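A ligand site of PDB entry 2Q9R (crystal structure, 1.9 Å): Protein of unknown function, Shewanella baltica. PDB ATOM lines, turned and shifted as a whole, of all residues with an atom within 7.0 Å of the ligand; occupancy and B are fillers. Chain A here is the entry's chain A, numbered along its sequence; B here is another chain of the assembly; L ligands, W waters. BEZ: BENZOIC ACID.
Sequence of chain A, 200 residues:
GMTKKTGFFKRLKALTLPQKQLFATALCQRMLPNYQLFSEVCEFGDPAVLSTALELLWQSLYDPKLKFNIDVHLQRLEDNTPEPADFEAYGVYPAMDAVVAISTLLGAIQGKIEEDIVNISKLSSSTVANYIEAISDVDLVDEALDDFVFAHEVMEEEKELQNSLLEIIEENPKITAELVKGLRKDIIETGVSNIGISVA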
ATOM      1  N   ILE A 132      18.747  -7.321  15.015  1.00  0.00           N
ATOM      2  CA  ILE A 132      19.254  -6.163  15.774  1.00  0.00           C
ATOM      3  C   ILE A 132      18.427  -5.935  17.026  1.00  0.00           C
ATOM      4  O   ILE A 132      18.985  -5.747  18.110  1.00  0.00           O
ATOM      5  CB  ILE A 132      19.217  -4.900  14.933  1.00  0.00           C
ATOM      6  CG1 ILE A 132      20.240  -5.000  13.773  1.00  0.00           C
ATOM      7  CG2 ILE A 132      19.470  -3.656  15.816  1.00  0.00           C
ATOM      8  CD1 ILE A 132      20.087  -3.959  12.683  1.00  0.00           C
ATOM      9  N   ILE A 135      18.615  -8.472  20.402  1.00  0.00           N
ATOM     10  CA  ILE A 135      19.675  -8.288  21.385  1.00  0.00           C
ATOM     11  C   ILE A 135      19.460  -6.976  22.161  1.00  0.00           C
ATOM     12  O   ILE A 135      19.483  -6.946  23.391  1.00  0.00           O
ATOM     13  CB  ILE A 135      21.030  -8.318  20.617  1.00  0.00           C
ATOM     14  CG1 ILE A 135      22.183  -7.578  21.348  1.00  0.00           C
ATOM     15  CG2 ILE A 135      20.806  -7.755  19.253  1.00  0.00           C
ATOM     16  N   SER A 136      19.179  -5.914  21.422  1.00  0.00           N
ATOM     17  CA  SER A 136      19.172  -4.556  21.953  1.00  0.00           C
ATOM     18  C   SER A 136      18.401  -4.300  23.228  1.00  0.00           C
ATOM     19  O   SER A 136      18.878  -3.632  24.141  1.00  0.00           O
ATOM     20  CB  SER A 136      18.651  -3.628  20.873  1.00  0.00           C
ATOM     21  OG  SER A 136      19.620  -3.495  19.838  1.00  0.00           O
ATOM     22  N   ASP A 137      17.152  -4.760  23.231  1.00  0.00           N
ATOM     23  CA  ASP A 137      16.257  -4.588  24.378  1.00  0.00           C
ATOM     24  C   ASP A 137      16.155  -3.116  24.771  1.00  0.00           C
ATOM     25  O   ASP A 137      16.334  -2.753  25.926  1.00  0.00           O
ATOM     26  CB  ASP A 137      16.762  -5.439  25.525  1.00  0.00           C
ATOM     27  CG  ASP A 137      15.646  -5.898  26.467  1.00  0.00           C
ATOM     28  OD1 ASP A 137      14.458  -5.494  26.308  1.00  0.00           O
ATOM     29  OD2 ASP A 137      15.985  -6.664  27.392  1.00  0.00           O
ATOM     30  N   VAL A 138      15.898  -2.275  23.777  1.00  0.00           N
ATOM     31  CA  VAL A 138      15.684  -0.843  24.004  1.00  0.00           C
ATOM     32  C   VAL A 138      14.202  -0.496  24.003  1.00  0.00           C
ATOM     33  O   VAL A 138      13.379  -1.219  23.428  1.00  0.00           O
ATOM     34  CB  VAL A 138      16.398   0.055  22.948  1.00  0.00           C
ATOM     35  CG1 VAL A 138      17.873  -0.032  23.090  1.00  0.00           C
ATOM     36  CG2 VAL A 138      15.957  -0.285  21.522  1.00  0.00           C
ATOM     37  N   PHE A 148      18.009   4.113  15.436  1.00  0.00           N
ATOM     38  CA  PHE A 148      18.815   3.187  16.218  1.00  0.00           C
ATOM     39  C   PHE A 148      19.134   1.922  15.428  1.00  0.00           C
ATOM     40  O   PHE A 148      20.274   1.468  15.383  1.00  0.00           O
ATOM     41  CB  PHE A 148      18.079   2.810  17.500  1.00  0.00           C
ATOM     42  CG  PHE A 148      18.768   1.771  18.300  1.00  0.00           C
ATOM     43  CD1 PHE A 148      19.803   2.115  19.147  1.00  0.00           C
ATOM     44  CD2 PHE A 148      18.388   0.442  18.211  1.00  0.00           C
ATOM     45  CE1 PHE A 148      20.455   1.132  19.891  1.00  0.00           C
ATOM     46  CE2 PHE A 148      19.009  -0.529  18.963  1.00  0.00           C
ATOM     47  CZ  PHE A 148      20.059  -0.198  19.790  1.00  0.00           C
ATOM     48  N   HIS A 152      23.311   0.374  12.870  1.00  0.00           N
ATOM     49  CA  HIS A 152      23.984  -0.916  12.832  1.00  0.00           C
ATOM     50  C   HIS A 152      24.355  -1.234  11.399  1.00  0.00           C
ATOM     51  O   HIS A 152      23.526  -1.206  10.539  1.00  0.00           O
ATOM     52  CB  HIS A 152      23.054  -2.003  13.342  1.00  0.00           C
ATOM     53  CG  HIS A 152      22.767  -1.905  14.814  1.00  0.00           C
ATOM     54  ND1 HIS A 152      22.013  -0.889  15.355  1.00  0.00           N
ATOM     55  CD2 HIS A 152      23.118  -2.713  15.847  1.00  0.00           C
ATOM     56  CE1 HIS A 152      21.957  -1.050  16.662  1.00  0.00           C
ATOM     57  NE2 HIS A 152      22.609  -2.150  16.983  1.00  0.00           N
ATOM     58  N   PRO B  33      32.169   4.523  19.085  1.00  0.00           N
ATOM     59  CA  PRO B  33      30.740   4.591  18.740  1.00  0.00           C
ATOM     60  C   PRO B  33      29.815   3.787  19.635  1.00  0.00           C
ATOM     61  O   PRO B  33      28.656   4.151  19.836  1.00  0.00           O
ATOM     62  CB  PRO B  33      30.716   4.060  17.313  1.00  0.00           C
ATOM     63  CG  PRO B  33      32.069   4.441  16.771  1.00  0.00           C
ATOM     64  CD  PRO B  33      32.993   4.183  17.916  1.00  0.00           C
ATOM     65  N   ASN B  34      30.320   2.679  20.182  1.00  0.00           N
ATOM     66  CA  ASN B  34      29.537   1.888  21.065  1.00  0.00           C
ATOM     67  C   ASN B  34      29.149   2.706  22.302  1.00  0.00           C
ATOM     68  O   ASN B  34      28.008   2.662  22.758  1.00  0.00           O
ATOM     69  CB  ASN B  34      30.315   0.637  21.481  1.00  0.00           C
ATOM     70  CG  ASN B  34      30.632  -0.296  20.318  1.00  0.00           C
ATOM     71  OD1 ASN B  34      29.927  -0.362  19.292  1.00  0.00           O
ATOM     72  ND2 ASN B  34      31.714  -1.060  20.486  1.00  0.00           N
ATOM     73  N   TYR B  35      30.103   3.428  22.865  1.00  0.00           N
ATOM     74  CA  TYR B  35      29.830   4.238  24.064  1.00  0.00           C
ATOM     75  C   TYR B  35      28.899   5.385  23.682  1.00  0.00           C
ATOM     76  O   TYR B  35      27.894   5.659  24.349  1.00  0.00           O
ATOM     77  CB  TYR B  35      31.124   4.706  24.741  1.00  0.00           C
ATOM     78  CG  TYR B  35      30.847   5.381  26.027  1.00  0.00           C
ATOM     79  CD1 TYR B  35      30.396   6.720  26.058  1.00  0.00           C
ATOM     80  CD2 TYR B  35      30.978   4.706  27.236  1.00  0.00           C
ATOM     81  CE1 TYR B  35      30.108   7.327  27.209  1.00  0.00           C
ATOM     82  CE2 TYR B  35      30.707   5.329  28.431  1.00  0.00           C
ATOM     83  CZ  TYR B  35      30.270   6.640  28.411  1.00  0.00           C
ATOM     84  OH  TYR B  35      29.975   7.230  29.590  1.00  0.00           O
ATOM     85  N   GLN B  36      29.163   5.987  22.527  1.00  0.00           N
ATOM     86  CA  GLN B  36      28.371   7.117  22.071  1.00  0.00           C
ATOM     87  C   GLN B  36      26.904   6.712  21.893  1.00  0.00           C
ATOM     88  O   GLN B  36      26.006   7.439  22.317  1.00  0.00           O
ATOM     89  CB  GLN B  36      28.931   7.681  20.761  1.00  0.00           C
ATOM     90  CG  GLN B  36      30.241   8.419  20.941  1.00  0.00           C
ATOM     91  CD  GLN B  36      30.911   8.723  19.637  1.00  0.00           C
ATOM     92  OE1 GLN B  36      30.926   7.897  18.737  1.00  0.00           O
ATOM     93  NE2 GLN B  36      31.507   9.899  19.540  1.00  0.00           N
ATOM     94  N   LEU B  37      26.675   5.586  21.260  1.00  0.00           N
ATOM     95  CA  LEU B  37      25.314   5.147  21.003  1.00  0.00           C
ATOM     96  C   LEU B  37      24.586   4.856  22.336  1.00  0.00           C
ATOM     97  O   LEU B  37      23.487   5.320  22.564  1.00  0.00           O
ATOM     98  CB  LEU B  37      25.277   3.919  20.072  1.00  0.00           C
ATOM     99  CG  LEU B  37      23.839   3.494  19.629  1.00  0.00           C
ATOM    100  CD1 LEU B  37      23.128   4.638  18.903  1.00  0.00           C
ATOM    101  CD2 LEU B  37      23.859   2.194  18.799  1.00  0.00           C
ATOM    102  N   PHE B  38      25.208   4.062  23.192  1.00  0.00           N
ATOM    103  CA  PHE B  38      24.642   3.743  24.472  1.00  0.00           C
ATOM    104  C   PHE B  38      24.269   5.017  25.266  1.00  0.00           C
ATOM    105  O   PHE B  38      23.200   5.110  25.885  1.00  0.00           O
ATOM    106  CB  PHE B  38      25.593   2.873  25.285  1.00  0.00           C
ATOM    107  CG  PHE B  38      25.204   2.745  26.731  1.00  0.00           C
ATOM    108  CD1 PHE B  38      24.119   1.972  27.086  1.00  0.00           C
ATOM    109  CD2 PHE B  38      25.891   3.420  27.728  1.00  0.00           C
ATOM    110  CE1 PHE B  38      23.751   1.840  28.381  1.00  0.00           C
ATOM    111  CE2 PHE B  38      25.502   3.284  29.070  1.00  0.00           C
ATOM    112  CZ  PHE B  38      24.445   2.494  29.386  1.00  0.00           C
ATOM    113  N   SER B  39      25.190   5.959  25.267  1.00  0.00           N
ATOM    114  CA  SER B  39      25.078   7.149  26.082  1.00  0.00           C
ATOM    115  C   SER B  39      23.883   7.966  25.653  1.00  0.00           C
ATOM    116  O   SER B  39      23.166   8.542  26.475  1.00  0.00           O
ATOM    117  CB  SER B  39      26.378   7.979  25.973  1.00  0.00           C
ATOM    118  OG  SER B  39      26.211   9.239  26.599  1.00  0.00           O
ATOM    119  N   VAL B  41      21.258   6.782  23.765  1.00  0.00           N
ATOM    120  CA  VAL B  41      20.042   6.016  23.905  1.00  0.00           C
ATOM    121  C   VAL B  41      19.626   5.850  25.357  1.00  0.00           C
ATOM    122  O   VAL B  41      18.473   5.955  25.695  1.00  0.00           O
ATOM    123  CB  VAL B  41      20.189   4.619  23.215  1.00  0.00           C
ATOM    124  CG1 VAL B  41      18.969   3.688  23.532  1.00  0.00           C
ATOM    125  CG2 VAL B  41      20.387   4.824  21.704  1.00  0.00           C
ATOM    126  N   CYS B  42      20.566   5.530  26.225  1.00  0.00           N
ATOM    127  CA  CYS B  42      20.231   5.261  27.606  1.00  0.00           C
ATOM    128  C   CYS B  42      20.422   6.483  28.527  1.00  0.00           C
ATOM    129  O   CYS B  42      20.201   6.375  29.716  1.00  0.00           O
ATOM    130  CB  CYS B  42      21.030   4.070  28.109  1.00  0.00           C
ATOM    131  SG  CYS B  42      20.513   2.520  27.313  1.00  0.00           S
ATOM    132  N   ALA B  89      19.001  -2.406  28.625  1.00  0.00           N
ATOM    133  CA  ALA B  89      19.537  -2.400  27.260  1.00  0.00           C
ATOM    134  C   ALA B  89      20.877  -3.131  27.200  1.00  0.00           C
ATOM    135  O   ALA B  89      21.694  -3.003  28.097  1.00  0.00           O
ATOM    136  CB  ALA B  89      19.654  -0.985  26.744  1.00  0.00           C
ATOM    137  N   TYR B  90      21.082  -3.910  26.130  1.00  0.00           N
ATOM    138  CA  TYR B  90      22.305  -4.678  25.926  1.00  0.00           C
ATOM    139  C   TYR B  90      23.545  -3.748  25.824  1.00  0.00           C
ATOM    140  O   TYR B  90      24.654  -4.119  26.232  1.00  0.00           O
ATOM    141  CB  TYR B  90      22.239  -5.610  24.665  1.00  0.00           C
ATOM    142  CG  TYR B  90      23.512  -6.414  24.532  1.00  0.00           C
ATOM    143  CD1 TYR B  90      23.733  -7.532  25.325  1.00  0.00           C
ATOM    144  CD2 TYR B  90      24.534  -5.980  23.707  1.00  0.00           C
ATOM    145  CE1 TYR B  90      24.916  -8.255  25.261  1.00  0.00           C
ATOM    146  CE2 TYR B  90      25.731  -6.678  23.638  1.00  0.00           C
ATOM    147  CZ  TYR B  90      25.939  -7.800  24.432  1.00  0.00           C
ATOM    148  OH  TYR B  90      27.123  -8.486  24.345  1.00  0.00           O
ATOM    149  N   GLY B  91      23.332  -2.551  25.256  1.00  0.00           N
ATOM    150  CA  GLY B  91      24.421  -1.596  24.984  1.00  0.00           C
ATOM    151  C   GLY B  91      25.297  -1.257  26.177  1.00  0.00           C
ATOM    152  O   GLY B  91      26.468  -0.851  26.012  1.00  0.00           O
ATOM    153  N   VAL B  92      24.786  -1.432  27.383  1.00  0.00           N
ATOM    154  CA  VAL B  92      25.614  -1.235  28.553  1.00  0.00           C
ATOM    155  C   VAL B  92      26.911  -2.052  28.458  1.00  0.00           C
ATOM    156  O   VAL B  92      27.965  -1.588  28.868  1.00  0.00           O
ATOM    157  CB  VAL B  92      24.851  -1.534  29.884  1.00  0.00           C
ATOM    158  CG1 VAL B  92      24.482  -3.042  30.003  1.00  0.00           C
ATOM    159  CG2 VAL B  92      25.663  -1.022  31.083  1.00  0.00           C
ATOM    160  N   PRO B  94      28.798  -3.379  25.579  1.00  0.00           N
ATOM    161  CA  PRO B  94      29.859  -2.756  24.786  1.00  0.00           C
ATOM    162  C   PRO B  94      30.332  -1.361  25.241  1.00  0.00           C
ATOM    163  O   PRO B  94      31.520  -1.025  25.076  1.00  0.00           O
ATOM    164  CB  PRO B  94      29.279  -2.726  23.349  1.00  0.00           C
ATOM    165  CG  PRO B  94      27.854  -3.129  23.441  1.00  0.00           C
ATOM    166  CD  PRO B  94      27.604  -3.720  24.801  1.00  0.00           C
ATOM    167  N   ALA B  95      29.425  -0.548  25.792  1.00  0.00           N
ATOM    168  CA  ALA B  95      29.784   0.763  26.329  1.00  0.00           C
ATOM    169  C   ALA B  95      30.795   0.621  27.462  1.00  0.00           C
ATOM    170  O   ALA B  95      31.820   1.294  27.460  1.00  0.00           O
ATOM    171  CB  ALA B  95      28.547   1.544  26.794  1.00  0.00           C
ATOM    172  N   TYR B 131      28.434 -10.141  21.774  1.00  0.00           N
ATOM    173  CA  TYR B 131      27.360  -9.618  20.940  1.00  0.00           C
ATOM    174  C   TYR B 131      26.692 -10.734  20.162  1.00  0.00           C
ATOM    175  O   TYR B 131      25.474 -10.874  20.215  1.00  0.00           O
ATOM    176  CB  TYR B 131      27.891  -8.542  19.989  1.00  0.00           C
ATOM    177  CG  TYR B 131      26.837  -7.928  19.100  1.00  0.00           C
ATOM    178  CD1 TYR B 131      25.944  -7.012  19.622  1.00  0.00           C
ATOM    179  CD2 TYR B 131      26.722  -8.256  17.749  1.00  0.00           C
ATOM    180  CE1 TYR B 131      24.971  -6.455  18.832  1.00  0.00           C
ATOM    181  CE2 TYR B 131      25.733  -7.699  16.947  1.00  0.00           C
ATOM    182  CZ  TYR B 131      24.875  -6.783  17.506  1.00  0.00           C
ATOM    183  OH  TYR B 131      23.890  -6.184  16.799  1.00  0.00           O
ATOM    184  N   SER B 193      32.251   0.671  14.614  1.00  0.00           N
ATOM    185  CA  SER B 193      32.829   0.009  15.780  1.00  0.00           C
ATOM    186  C   SER B 193      33.097  -1.447  15.480  1.00  0.00           C
ATOM    187  O   SER B 193      32.695  -1.958  14.448  1.00  0.00           O
ATOM    188  CB  SER B 193      31.910   0.087  17.003  1.00  0.00           C
ATOM    189  OG  SER B 193      30.875  -0.893  17.011  1.00  0.00           O
ATOM    190  N   ILE B 195      31.593  -3.813  16.673  1.00  0.00           N
ATOM    191  CA  ILE B 195      30.307  -4.525  16.544  1.00  0.00           C
ATOM    192  C   ILE B 195      29.349  -3.835  15.547  1.00  0.00           C
ATOM    193  O   ILE B 195      28.118  -4.056  15.573  1.00  0.00           O
ATOM    194  CB  ILE B 195      29.644  -4.858  17.892  1.00  0.00           C
ATOM    195  CG1 ILE B 195      29.428  -3.623  18.780  1.00  0.00           C
ATOM    196  CG2 ILE B 195      30.434  -5.909  18.655  1.00  0.00           C
ATOM    197  CD1 ILE B 195      28.301  -3.886  19.824  1.00  0.00           C
ATOM    198  N   ILE B 197      28.679  -0.538  14.917  1.00  0.00           N
ATOM    199  CA  ILE B 197      27.976   0.695  15.281  1.00  0.00           C
ATOM    200  C   ILE B 197      28.602   1.927  14.667  1.00  0.00           C
ATOM    201  O   ILE B 197      29.838   2.175  14.717  1.00  0.00           O
ATOM    202  CB  ILE B 197      27.913   0.857  16.829  1.00  0.00           C
ATOM    203  CG1 ILE B 197      27.178  -0.356  17.438  1.00  0.00           C
ATOM    204  CG2 ILE B 197      27.253   2.190  17.157  1.00  0.00           C
ATOM    205  CD1 ILE B 197      25.748  -0.527  16.891  1.00  0.00           C
HETATM  206  C   BEZ L   1      22.936  -2.488  20.539  1.00  0.00           C
HETATM  207  O1  BEZ L   1      23.040  -3.008  19.382  1.00  0.00           O
HETATM  208  O2  BEZ L   1      21.999  -2.781  21.335  1.00  0.00           O
HETATM  209  C1  BEZ L   1      23.963  -1.491  20.975  1.00  0.00           C
HETATM  210  C2  BEZ L   1      23.565  -0.365  21.748  1.00  0.00           C
HETATM  211  C3  BEZ L   1      24.539   0.548  22.129  1.00  0.00           C
HETATM  212  C4  BEZ L   1      25.874   0.352  21.768  1.00  0.00           C
HETATM  213  C5  BEZ L   1      26.243  -0.764  21.016  1.00  0.00           C
HETATM  214  C6  BEZ L   1      25.283  -1.713  20.620  1.00  0.00           C
HETATM  215  O   HOH W   1      20.955  -1.879  23.597  1.00  0.00           O
HETATM  216  O   HOH W   2      21.789  -5.229  18.244  1.00  0.00           O
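NE2 of His 152 is in hydrogen-bond range of O1 of the ligand.
The side-chain hydroxyl (OG) of Ser 136 sits at hydrogen-bond distance from an oxygen (O2) of the ligand, at 2.9 Å.
OD1 of Asn 34 of chain B lies within hydrogen-bond range of OG of Ser 193 of chain B (2.5 Å).
The backbone carbonyl oxygen of Ile 132 is in hydrogen-bond range of the side-chain hydroxyl of Ser 136 (2.9 Å).
OG of Ser 193 of chain B lies within hydrogen-bond range of N of Ile 195 of chain B (3.0 Å).
The backbone carbonyl oxygen (O) of Ser 136 is in hydrogen-bond range of the backbone NH (N) of Tyr 90 of chain B.
A ring nitrogen (ND1) of His 152 is in hydrogen-bond range of the backbone carbonyl oxygen (O) of Phe 148 (2.9 Å).
N of Ile 197 of chain B lies within hydrogen-bond range of OG of Ser 193 of chain B, 3.1 Å away.
The backbone NH (N) of Tyr 131 of chain B sits at hydrogen-bond distance from the side-chain hydroxyl (OH) of Tyr 90 of chain B (3.3 Å).
Residues that only touch the ligand: Phe 148 (3.6 Å), Asn 34 of chain B (3.3 Å), Leu 37 of chain B (3.8 Å), Phe 38 of chain B (3.7 Å), Gly 91 of chain B (3.6 Å), Pro 94 of chain B (3.8 Å), Tyr 131 of chain B (3.99 Å), Ile 195 of chain B (3.8 Å) and Ile 197 of chain B (3.7 Å).
11 residues have an atom within 4 Å of the ligand: Ser 136, Phe 148, His 152, Asn 34 of chain B, Leu 37 of chain B, Phe 38 of chain B, Gly 91 of chain B, Pro 94 of chain B, Tyr 131 of chain B, Ile 195 of chain B and Ile 197 of chain B.
Water W1 lies within hydrogen-bond range of an oxygen (O2) of the ligand, the backbone carbonyl oxygen of Ser 136, the backbone NH of Gly 91 of chain B and the backbone NH of Tyr 90 of chain B.
Water W2 lies within hydrogen-bond range of OH of Tyr 131 of chain B (2.7 Å), O1 of the ligand (2.8 Å), O of Ile 132 (2.9 Å), OG of Ser 136 (3.2 Å) and NE2 of His 152 (3.4 Å).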
